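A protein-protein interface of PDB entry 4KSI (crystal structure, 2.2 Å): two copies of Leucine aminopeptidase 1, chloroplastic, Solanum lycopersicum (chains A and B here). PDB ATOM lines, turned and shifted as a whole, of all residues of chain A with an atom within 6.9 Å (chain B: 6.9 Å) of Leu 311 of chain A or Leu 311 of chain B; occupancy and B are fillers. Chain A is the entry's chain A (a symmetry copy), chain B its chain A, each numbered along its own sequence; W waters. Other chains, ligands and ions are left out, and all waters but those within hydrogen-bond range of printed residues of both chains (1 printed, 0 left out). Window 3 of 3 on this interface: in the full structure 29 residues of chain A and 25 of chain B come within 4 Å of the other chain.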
ATOM      1  N   SER A 306       5.410 -18.750 -11.489  1.00  0.00           N
ATOM      2  CA  SER A 306       5.788 -18.076 -12.733  1.00  0.00           C
ATOM      3  C   SER A 306       5.798 -16.551 -12.510  1.00  0.00           C
ATOM      4  O   SER A 306       6.295 -15.851 -13.339  1.00  0.00           O
ATOM      5  CB  SER A 306       4.800 -18.413 -13.875  1.00  0.00           C
ATOM      6  OG  SER A 306       3.492 -17.883 -13.565  1.00  0.00           O
ATOM      7  N   GLY A 307       5.182 -16.042 -11.437  1.00  0.00           N
ATOM      8  CA  GLY A 307       4.895 -14.596 -11.354  1.00  0.00           C
ATOM      9  C   GLY A 307       3.444 -14.287 -11.700  1.00  0.00           C
ATOM     10  O   GLY A 307       2.923 -13.225 -11.329  1.00  0.00           O
ATOM     11  N   GLY A 308       2.752 -15.206 -12.401  1.00  0.00           N
ATOM     12  CA  GLY A 308       1.365 -14.942 -12.857  1.00  0.00           C
ATOM     13  C   GLY A 308       1.447 -13.888 -13.951  1.00  0.00           C
ATOM     14  O   GLY A 308       2.488 -13.783 -14.651  1.00  0.00           O
ATOM     15  N   TYR A 309       0.375 -13.091 -14.132  1.00  0.00           N
ATOM     16  CA  TYR A 309       0.437 -12.027 -15.168  1.00  0.00           C
ATOM     17  C   TYR A 309       1.649 -11.057 -15.031  1.00  0.00           C
ATOM     18  O   TYR A 309       2.151 -10.532 -16.044  1.00  0.00           O
ATOM     19  CB  TYR A 309      -0.889 -11.251 -15.304  1.00  0.00           C
ATOM     20  CG  TYR A 309      -1.865 -12.046 -16.192  1.00  0.00           C
ATOM     21  CD1 TYR A 309      -1.764 -11.990 -17.606  1.00  0.00           C
ATOM     22  CD2 TYR A 309      -2.816 -12.898 -15.624  1.00  0.00           C
ATOM     23  CE1 TYR A 309      -2.619 -12.757 -18.433  1.00  0.00           C
ATOM     24  CE2 TYR A 309      -3.684 -13.645 -16.435  1.00  0.00           C
ATOM     25  CZ  TYR A 309      -3.575 -13.580 -17.846  1.00  0.00           C
ATOM     26  OH  TYR A 309      -4.420 -14.348 -18.632  1.00  0.00           O
ATOM     27  N   ASN A 310       2.116 -10.847 -13.799  1.00  0.00           N
ATOM     28  CA  ASN A 310       3.381 -10.164 -13.589  1.00  0.00           C
ATOM     29  C   ASN A 310       4.498 -11.215 -13.756  1.00  0.00           C
ATOM     30  O   ASN A 310       5.283 -11.506 -12.821  1.00  0.00           O
ATOM     31  CB  ASN A 310       3.397  -9.536 -12.187  1.00  0.00           C
ATOM     32  CG  ASN A 310       2.628  -8.192 -12.132  1.00  0.00           C
ATOM     33  OD1 ASN A 310       3.122  -7.119 -12.624  1.00  0.00           O
ATOM     34  ND2 ASN A 310       1.473  -8.220 -11.538  1.00  0.00           N
ATOM     35  N   LEU A 311       4.561 -11.799 -14.937  1.00  0.00           N
ATOM     36  CA  LEU A 311       5.516 -12.861 -15.262  1.00  0.00           C
ATOM     37  C   LEU A 311       6.980 -12.467 -14.873  1.00  0.00           C
ATOM     38  O   LEU A 311       7.448 -11.326 -15.174  1.00  0.00           O
ATOM     39  CB  LEU A 311       5.475 -13.065 -16.800  1.00  0.00           C
ATOM     40  CG  LEU A 311       6.323 -14.238 -17.330  1.00  0.00           C
ATOM     41  CD1 LEU A 311       5.963 -15.622 -16.721  1.00  0.00           C
ATOM     42  CD2 LEU A 311       6.174 -14.215 -18.855  1.00  0.00           C
ATOM     43  N   LYS A 312       7.691 -13.413 -14.268  1.00  0.00           N
ATOM     44  CA  LYS A 312       9.137 -13.272 -14.023  1.00  0.00           C
ATOM     45  C   LYS A 312       9.925 -13.203 -15.332  1.00  0.00           C
ATOM     46  O   LYS A 312       9.949 -14.167 -16.107  1.00  0.00           O
ATOM     47  CB  LYS A 312       9.587 -14.470 -13.179  1.00  0.00           C
ATOM     48  CG  LYS A 312       9.085 -14.422 -11.742  1.00  0.00           C
ATOM     49  CD  LYS A 312       9.473 -15.691 -10.979  1.00  0.00           C
ATOM     50  CE  LYS A 312       8.864 -15.711  -9.559  1.00  0.00           C
ATOM     51  NZ  LYS A 312       9.374 -14.481  -8.816  1.00  0.00           N
ATOM     52  N   VAL A 313      10.471 -12.047 -15.652  1.00  0.00           N
ATOM     53  CA  VAL A 313      11.203 -11.828 -16.923  1.00  0.00           C
ATOM     54  C   VAL A 313      12.578 -11.198 -16.637  1.00  0.00           C
ATOM     55  O   VAL A 313      12.811 -10.689 -15.545  1.00  0.00           O
ATOM     56  CB  VAL A 313      10.418 -10.905 -17.913  1.00  0.00           C
ATOM     57  CG1 VAL A 313       9.152 -11.577 -18.350  1.00  0.00           C
ATOM     58  CG2 VAL A 313      10.170  -9.516 -17.285  1.00  0.00           C
ATOM     59  N   GLY A 314      13.479 -11.177 -17.622  1.00  0.00           N
ATOM     60  CA  GLY A 314      14.895 -10.760 -17.342  1.00  0.00           C
ATOM     61  C   GLY A 314      15.852 -11.946 -17.179  1.00  0.00           C
ATOM     62  O   GLY A 314      15.439 -13.083 -16.793  1.00  0.00           O
ATOM     63  N   SER A 317      15.879 -13.556 -13.634  1.00  0.00           N
ATOM     64  CA  SER A 317      14.560 -13.752 -13.056  1.00  0.00           C
ATOM     65  C   SER A 317      14.583 -14.993 -12.139  1.00  0.00           C
ATOM     66  O   SER A 317      13.734 -15.099 -11.238  1.00  0.00           O
ATOM     67  CB  SER A 317      13.513 -13.981 -14.164  1.00  0.00           C
ATOM     68  OG  SER A 317      13.632 -15.308 -14.726  1.00  0.00           O
ATOM     69  N   ILE A 319      13.376 -17.695 -12.911  1.00  0.00           N
ATOM     70  CA  ILE A 319      12.085 -18.414 -13.065  1.00  0.00           C
ATOM     71  C   ILE A 319      12.347 -19.921 -13.096  1.00  0.00           C
ATOM     72  O   ILE A 319      11.559 -20.660 -12.577  1.00  0.00           O
ATOM     73  CB  ILE A 319      11.262 -17.952 -14.288  1.00  0.00           C
ATOM     74  CG1 ILE A 319       9.798 -18.431 -14.165  1.00  0.00           C
ATOM     75  CG2 ILE A 319      11.971 -18.261 -15.638  1.00  0.00           C
ATOM     76  CD1 ILE A 319       8.977 -17.862 -15.351  1.00  0.00           C
ATOM     77  N   ILE A 360      -0.327 -18.884 -15.449  1.00  0.00           N
ATOM     78  CA  ILE A 360      -1.011 -17.925 -16.267  1.00  0.00           C
ATOM     79  C   ILE A 360      -2.061 -18.664 -17.049  1.00  0.00           C
ATOM     80  O   ILE A 360      -1.761 -19.684 -17.670  1.00  0.00           O
ATOM     81  CB  ILE A 360      -0.038 -17.239 -17.242  1.00  0.00           C
ATOM     82  CG1 ILE A 360       0.967 -16.338 -16.480  1.00  0.00           C
ATOM     83  CG2 ILE A 360      -0.802 -16.416 -18.291  1.00  0.00           C
ATOM     84  CD1 ILE A 360       2.057 -15.725 -17.390  1.00  0.00           C
ATOM     85  N   ASN A 383       0.750  -6.390  -7.764  1.00  0.00           N
ATOM     86  CA  ASN A 383       1.745  -7.224  -8.484  1.00  0.00           C
ATOM     87  C   ASN A 383       1.447  -8.684  -8.199  1.00  0.00           C
ATOM     88  O   ASN A 383       1.457  -9.081  -7.041  1.00  0.00           O
ATOM     89  CB  ASN A 383       3.199  -6.871  -8.053  1.00  0.00           C
ATOM     90  CG  ASN A 383       4.273  -7.535  -8.946  1.00  0.00           C
ATOM     91  OD1 ASN A 383       4.193  -8.734  -9.288  1.00  0.00           O
ATOM     92  ND2 ASN A 383       5.308  -6.746  -9.323  1.00  0.00           N
ATOM     93  N   THR A 384       1.136  -9.475  -9.209  1.00  0.00           N
ATOM     94  CA  THR A 384       0.738 -10.857  -8.937  1.00  0.00           C
ATOM     95  C   THR A 384       1.907 -11.741  -8.597  1.00  0.00           C
ATOM     96  O   THR A 384       1.716 -12.910  -8.283  1.00  0.00           O
ATOM     97  CB  THR A 384       0.001 -11.511 -10.146  1.00  0.00           C
ATOM     98  OG1 THR A 384       0.903 -11.603 -11.263  1.00  0.00           O
ATOM     99  CG2 THR A 384      -1.245 -10.652 -10.545  1.00  0.00           C
ATOM    100  N   ASP A 385       3.121 -11.205  -8.717  1.00  0.00           N
ATOM    101  CA  ASP A 385       4.302 -11.953  -8.349  1.00  0.00           C
ATOM    102  C   ASP A 385       4.636 -11.784  -6.845  1.00  0.00           C
ATOM    103  O   ASP A 385       5.632 -12.327  -6.331  1.00  0.00           O
ATOM    104  CB  ASP A 385       5.489 -11.551  -9.221  1.00  0.00           C
ATOM    105  CG  ASP A 385       6.679 -12.524  -9.062  1.00  0.00           C
ATOM    106  OD1 ASP A 385       6.547 -13.673  -8.490  1.00  0.00           O
ATOM    107  OD2 ASP A 385       7.755 -12.173  -9.506  1.00  0.00           O
ATOM    108  N   SER B 306      -4.062  -7.311 -20.428  1.00  0.00           N
ATOM    109  CA  SER B 306      -2.735  -7.791 -20.037  1.00  0.00           C
ATOM    110  C   SER B 306      -1.719  -7.457 -21.148  1.00  0.00           C
ATOM    111  O   SER B 306      -0.554  -7.568 -20.915  1.00  0.00           O
ATOM    112  CB  SER B 306      -2.739  -9.320 -19.800  1.00  0.00           C
ATOM    113  OG  SER B 306      -3.018 -10.009 -21.040  1.00  0.00           O
ATOM    114  N   GLY B 307      -2.165  -7.129 -22.366  1.00  0.00           N
ATOM    115  CA  GLY B 307      -1.245  -7.116 -23.522  1.00  0.00           C
ATOM    116  C   GLY B 307      -1.384  -8.375 -24.369  1.00  0.00           C
ATOM    117  O   GLY B 307      -0.997  -8.384 -25.546  1.00  0.00           O
ATOM    118  N   GLY B 308      -1.948  -9.459 -23.802  1.00  0.00           N
ATOM    119  CA  GLY B 308      -2.036 -10.750 -24.527  1.00  0.00           C
ATOM    120  C   GLY B 308      -0.622 -11.302 -24.629  1.00  0.00           C
ATOM    121  O   GLY B 308       0.239 -10.996 -23.763  1.00  0.00           O
ATOM    122  N   TYR B 309      -0.342 -12.116 -25.666  1.00  0.00           N
ATOM    123  CA  TYR B 309       1.041 -12.643 -25.814  1.00  0.00           C
ATOM    124  C   TYR B 309       2.152 -11.551 -25.840  1.00  0.00           C
ATOM    125  O   TYR B 309       3.289 -11.802 -25.397  1.00  0.00           O
ATOM    126  CB  TYR B 309       1.183 -13.615 -27.002  1.00  0.00           C
ATOM    127  CG  TYR B 309       0.703 -15.017 -26.583  1.00  0.00           C
ATOM    128  CD1 TYR B 309       1.557 -15.886 -25.857  1.00  0.00           C
ATOM    129  CD2 TYR B 309      -0.608 -15.432 -26.841  1.00  0.00           C
ATOM    130  CE1 TYR B 309       1.112 -17.157 -25.419  1.00  0.00           C
ATOM    131  CE2 TYR B 309      -1.051 -16.699 -26.432  1.00  0.00           C
ATOM    132  CZ  TYR B 309      -0.190 -17.557 -25.708  1.00  0.00           C
ATOM    133  OH  TYR B 309      -0.655 -18.792 -25.285  1.00  0.00           O
ATOM    134  N   ASN B 310       1.813 -10.357 -26.330  1.00  0.00           N
ATOM    135  CA  ASN B 310       2.692  -9.211 -26.175  1.00  0.00           C
ATOM    136  C   ASN B 310       2.431  -8.627 -24.771  1.00  0.00           C
ATOM    137  O   ASN B 310       2.004  -7.459 -24.606  1.00  0.00           O
ATOM    138  CB  ASN B 310       2.397  -8.186 -27.280  1.00  0.00           C
ATOM    139  CG  ASN B 310       3.071  -8.556 -28.625  1.00  0.00           C
ATOM    140  OD1 ASN B 310       4.328  -8.401 -28.808  1.00  0.00           O
ATOM    141  ND2 ASN B 310       2.282  -9.007 -29.554  1.00  0.00           N
ATOM    142  N   LEU B 311       2.667  -9.442 -23.761  1.00  0.00           N
ATOM    143  CA  LEU B 311       2.422  -9.083 -22.362  1.00  0.00           C
ATOM    144  C   LEU B 311       3.065  -7.704 -21.992  1.00  0.00           C
ATOM    145  O   LEU B 311       4.257  -7.432 -22.330  1.00  0.00           O
ATOM    146  CB  LEU B 311       3.098 -10.169 -21.481  1.00  0.00           C
ATOM    147  CG  LEU B 311       2.841 -10.039 -19.966  1.00  0.00           C
ATOM    148  CD1 LEU B 311       1.340 -10.055 -19.562  1.00  0.00           C
ATOM    149  CD2 LEU B 311       3.636 -11.169 -19.303  1.00  0.00           C
ATOM    150  N   LYS B 312       2.302  -6.887 -21.271  1.00  0.00           N
ATOM    151  CA  LYS B 312       2.830  -5.648 -20.673  1.00  0.00           C
ATOM    152  C   LYS B 312       3.900  -5.941 -19.622  1.00  0.00           C
ATOM    153  O   LYS B 312       3.617  -6.555 -18.586  1.00  0.00           O
ATOM    154  CB  LYS B 312       1.649  -4.890 -20.053  1.00  0.00           C
ATOM    155  CG  LYS B 312       0.706  -4.288 -21.086  1.00  0.00           C
ATOM    156  CD  LYS B 312      -0.507  -3.639 -20.413  1.00  0.00           C
ATOM    157  CE  LYS B 312      -1.533  -3.134 -21.452  1.00  0.00           C
ATOM    158  NZ  LYS B 312      -0.829  -2.120 -22.347  1.00  0.00           N
ATOM    159  N   VAL B 313       5.144  -5.622 -19.917  1.00  0.00           N
ATOM    160  CA  VAL B 313       6.284  -5.914 -19.013  1.00  0.00           C
ATOM    161  C   VAL B 313       7.124  -4.641 -18.798  1.00  0.00           C
ATOM    162  O   VAL B 313       6.994  -3.680 -19.548  1.00  0.00           O
ATOM    163  CB  VAL B 313       7.210  -7.046 -19.568  1.00  0.00           C
ATOM    164  CG1 VAL B 313       6.464  -8.344 -19.618  1.00  0.00           C
ATOM    165  CG2 VAL B 313       7.804  -6.645 -20.936  1.00  0.00           C
ATOM    166  N   GLY B 314       8.025  -4.640 -17.812  1.00  0.00           N
ATOM    167  CA  GLY B 314       8.725  -3.367 -17.431  1.00  0.00           C
ATOM    168  C   GLY B 314       8.122  -2.695 -16.193  1.00  0.00           C
ATOM    169  O   GLY B 314       6.907  -2.869 -15.869  1.00  0.00           O
ATOM    170  N   SER B 317       4.995  -0.483 -16.890  1.00  0.00           N
ATOM    171  CA  SER B 317       4.025  -1.083 -17.791  1.00  0.00           C
ATOM    172  C   SER B 317       2.610  -0.594 -17.420  1.00  0.00           C
ATOM    173  O   SER B 317       1.712  -0.624 -18.277  1.00  0.00           O
ATOM    174  CB  SER B 317       4.060  -2.620 -17.676  1.00  0.00           C
ATOM    175  OG  SER B 317       3.427  -3.064 -16.453  1.00  0.00           O
ATOM    176  N   ILE B 319       0.560  -2.309 -15.933  1.00  0.00           N
ATOM    177  CA  ILE B 319      -0.386  -3.441 -16.108  1.00  0.00           C
ATOM    178  C   ILE B 319      -1.389  -3.445 -14.953  1.00  0.00           C
ATOM    179  O   ILE B 319      -2.525  -3.760 -15.169  1.00  0.00           O
ATOM    180  CB  ILE B 319       0.310  -4.811 -16.264  1.00  0.00           C
ATOM    181  CG1 ILE B 319      -0.675  -5.856 -16.833  1.00  0.00           C
ATOM    182  CG2 ILE B 319       1.093  -5.234 -14.987  1.00  0.00           C
ATOM    183  CD1 ILE B 319       0.082  -7.187 -17.076  1.00  0.00           C
ATOM    184  N   ILE B 360      -4.197 -14.185 -21.587  1.00  0.00           N
ATOM    185  CA  ILE B 360      -3.299 -15.124 -22.194  1.00  0.00           C
ATOM    186  C   ILE B 360      -3.824 -16.503 -21.907  1.00  0.00           C
ATOM    187  O   ILE B 360      -4.127 -16.818 -20.756  1.00  0.00           O
ATOM    188  CB  ILE B 360      -1.882 -14.986 -21.612  1.00  0.00           C
ATOM    189  CG1 ILE B 360      -1.243 -13.634 -22.021  1.00  0.00           C
ATOM    190  CG2 ILE B 360      -0.989 -16.154 -22.058  1.00  0.00           C
ATOM    191  CD1 ILE B 360       0.130 -13.376 -21.356  1.00  0.00           C
ATOM    192  N   ASN B 383       1.298  -6.792 -33.052  1.00  0.00           N
ATOM    193  CA  ASN B 383       1.455  -6.643 -31.584  1.00  0.00           C
ATOM    194  C   ASN B 383       0.098  -6.839 -30.932  1.00  0.00           C
ATOM    195  O   ASN B 383      -0.828  -6.100 -31.243  1.00  0.00           O
ATOM    196  CB  ASN B 383       2.039  -5.248 -31.214  1.00  0.00           C
ATOM    197  CG  ASN B 383       2.447  -5.138 -29.726  1.00  0.00           C
ATOM    198  OD1 ASN B 383       1.712  -5.565 -28.810  1.00  0.00           O
ATOM    199  ND2 ASN B 383       3.637  -4.541 -29.474  1.00  0.00           N
ATOM    200  N   THR B 384      -0.056  -7.837 -30.080  1.00  0.00           N
ATOM    201  CA  THR B 384      -1.385  -8.105 -29.530  1.00  0.00           C
ATOM    202  C   THR B 384      -1.780  -7.123 -28.460  1.00  0.00           C
ATOM    203  O   THR B 384      -2.895  -7.188 -27.955  1.00  0.00           O
ATOM    204  CB  THR B 384      -1.493  -9.532 -28.909  1.00  0.00           C
ATOM    205  OG1 THR B 384      -0.604  -9.632 -27.783  1.00  0.00           O
ATOM    206  CG2 THR B 384      -1.115 -10.613 -29.977  1.00  0.00           C
ATOM    207  N   ASP B 385      -0.849  -6.252 -28.071  1.00  0.00           N
ATOM    208  CA  ASP B 385      -1.153  -5.227 -27.098  1.00  0.00           C
ATOM    209  C   ASP B 385      -1.723  -3.954 -27.773  1.00  0.00           C
ATOM    210  O   ASP B 385      -2.025  -2.943 -27.113  1.00  0.00           O
ATOM    211  CB  ASP B 385       0.079  -4.897 -26.259  1.00  0.00           C
ATOM    212  CG  ASP B 385      -0.275  -4.031 -25.029  1.00  0.00           C
ATOM    213  OD1 ASP B 385      -1.493  -3.878 -24.633  1.00  0.00           O
ATOM    214  OD2 ASP B 385       0.643  -3.501 -24.433  1.00  0.00           O
HETATM  215  O   HOH W   1       3.953  -8.242 -16.599  1.00  0.00           O
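The backbone NH of Ile 360 of chain B sits at hydrogen-bond distance from the side-chain hydroxyl of Tyr 309 of chain A (3.0 Å).
N of Gly 308 of chain B lies within hydrogen-bond range of OG of Ser 306 of chain B (3.0 Å). N of Lys 312 of chain B is in hydrogen-bond range of O of Ser 306 of chain B (3.0 Å). The side-chain hydroxyl (OG) of Ser 317 of chain B is in hydrogen-bond range of the backbone NH (N) of Ile 319 of chain B, 3.0 Å away. OG1 of Thr 384 of chain A lies within hydrogen-bond range of N of Tyr 309 of chain A. N of Thr 384 of chain A sits close to ND2 of Asn 310 of chain A (2.7 Å).
Among the printed residues, merely in contact across the chains: Tyr 309 of chain A with Ser 306 of chain B, Tyr 309 of chain A with Leu 311 of chain B, Leu 311 of chain A with Leu 311 of chain B, Asn 310 of chain A with Ile 319 of chain B and Ile 360 of chain A with Ile 360 of chain B.
Leu 311 of chain A touches one residue of chain B. Of the printed residues of chain A, Ser 306 of chain B touches Tyr 309. Of the printed residues of chain A, Ile 360 of chain B touches Tyr 309 (3.0 Å) and Ile 360 (3.8 Å). Printed residues of chain B within 4 Å of Asn 310 of chain A: Ile 319 (3.6 Å). Of the printed residues of chain B, Tyr 309 of chain A touches Ser 306, Leu 311 and Ile 360. Printed residues of chain B within 4 Å of Ile 360 of chain A: Ile 360 (3.8 Å). Lys 312 of chain A touches none of the printed residues of chain B. The nearest residue of chain B that does not touch Leu 311 of chain A is Val 313 of chain B (5.4 Å). The nearest residue of chain A that does not touch Leu 311 of chain B is Ile 360 of chain A (5.2 Å).
Of the 15 printed residues of chain B, 4 touch a printed residue of chain A. Printed residues of chain B that touch a printed residue of chain A: Ser 306, Leu 311, Ile 319 and Ile 360. Hydrophobic or aromatic side chains of chain B that line the printed part of chain A: Leu 311, Ile 319 and Ile 360. Hydrophobic or aromatic side chains of chain A within 4 Å of the printed part of chain B: Tyr 309, Leu 311 and Ile 360. Among the printed residues, no Asp or Glu carboxylate lies within 4 Å of a Lys or Arg side-chain nitrogen of the other chain.
Tyr 309 of chain A touches Ser 306 of chain B, but with the chains exchanged Ser 306 of chain A does not touch Tyr 309 of chain B (12.1 Å). Tyr 309 of chain A touches Ile 360 of chain B, but with the chains exchanged Ile 360 of chain A does not touch Tyr 309 of chain B (7.4 Å). Leu 311 of chain B touches its own counterpart, Leu 311 of chain A. Ile 360 of chain A touches its own counterpart, Ile 360 of chain B. Positions printed for both chains: 306, 307, 308, 309, 310, 311, 312, 313, 314, 317, 319, 360, 383, 384 and 385. Of the 6 pairs that touch across the chains among the printed residues, 2 have their exchanged pair printed and touching as well.
Water W1 bridges O of Lys 312 of chain B (2.6 Å) and O of Tyr 309 of chain A (3.0 Å).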
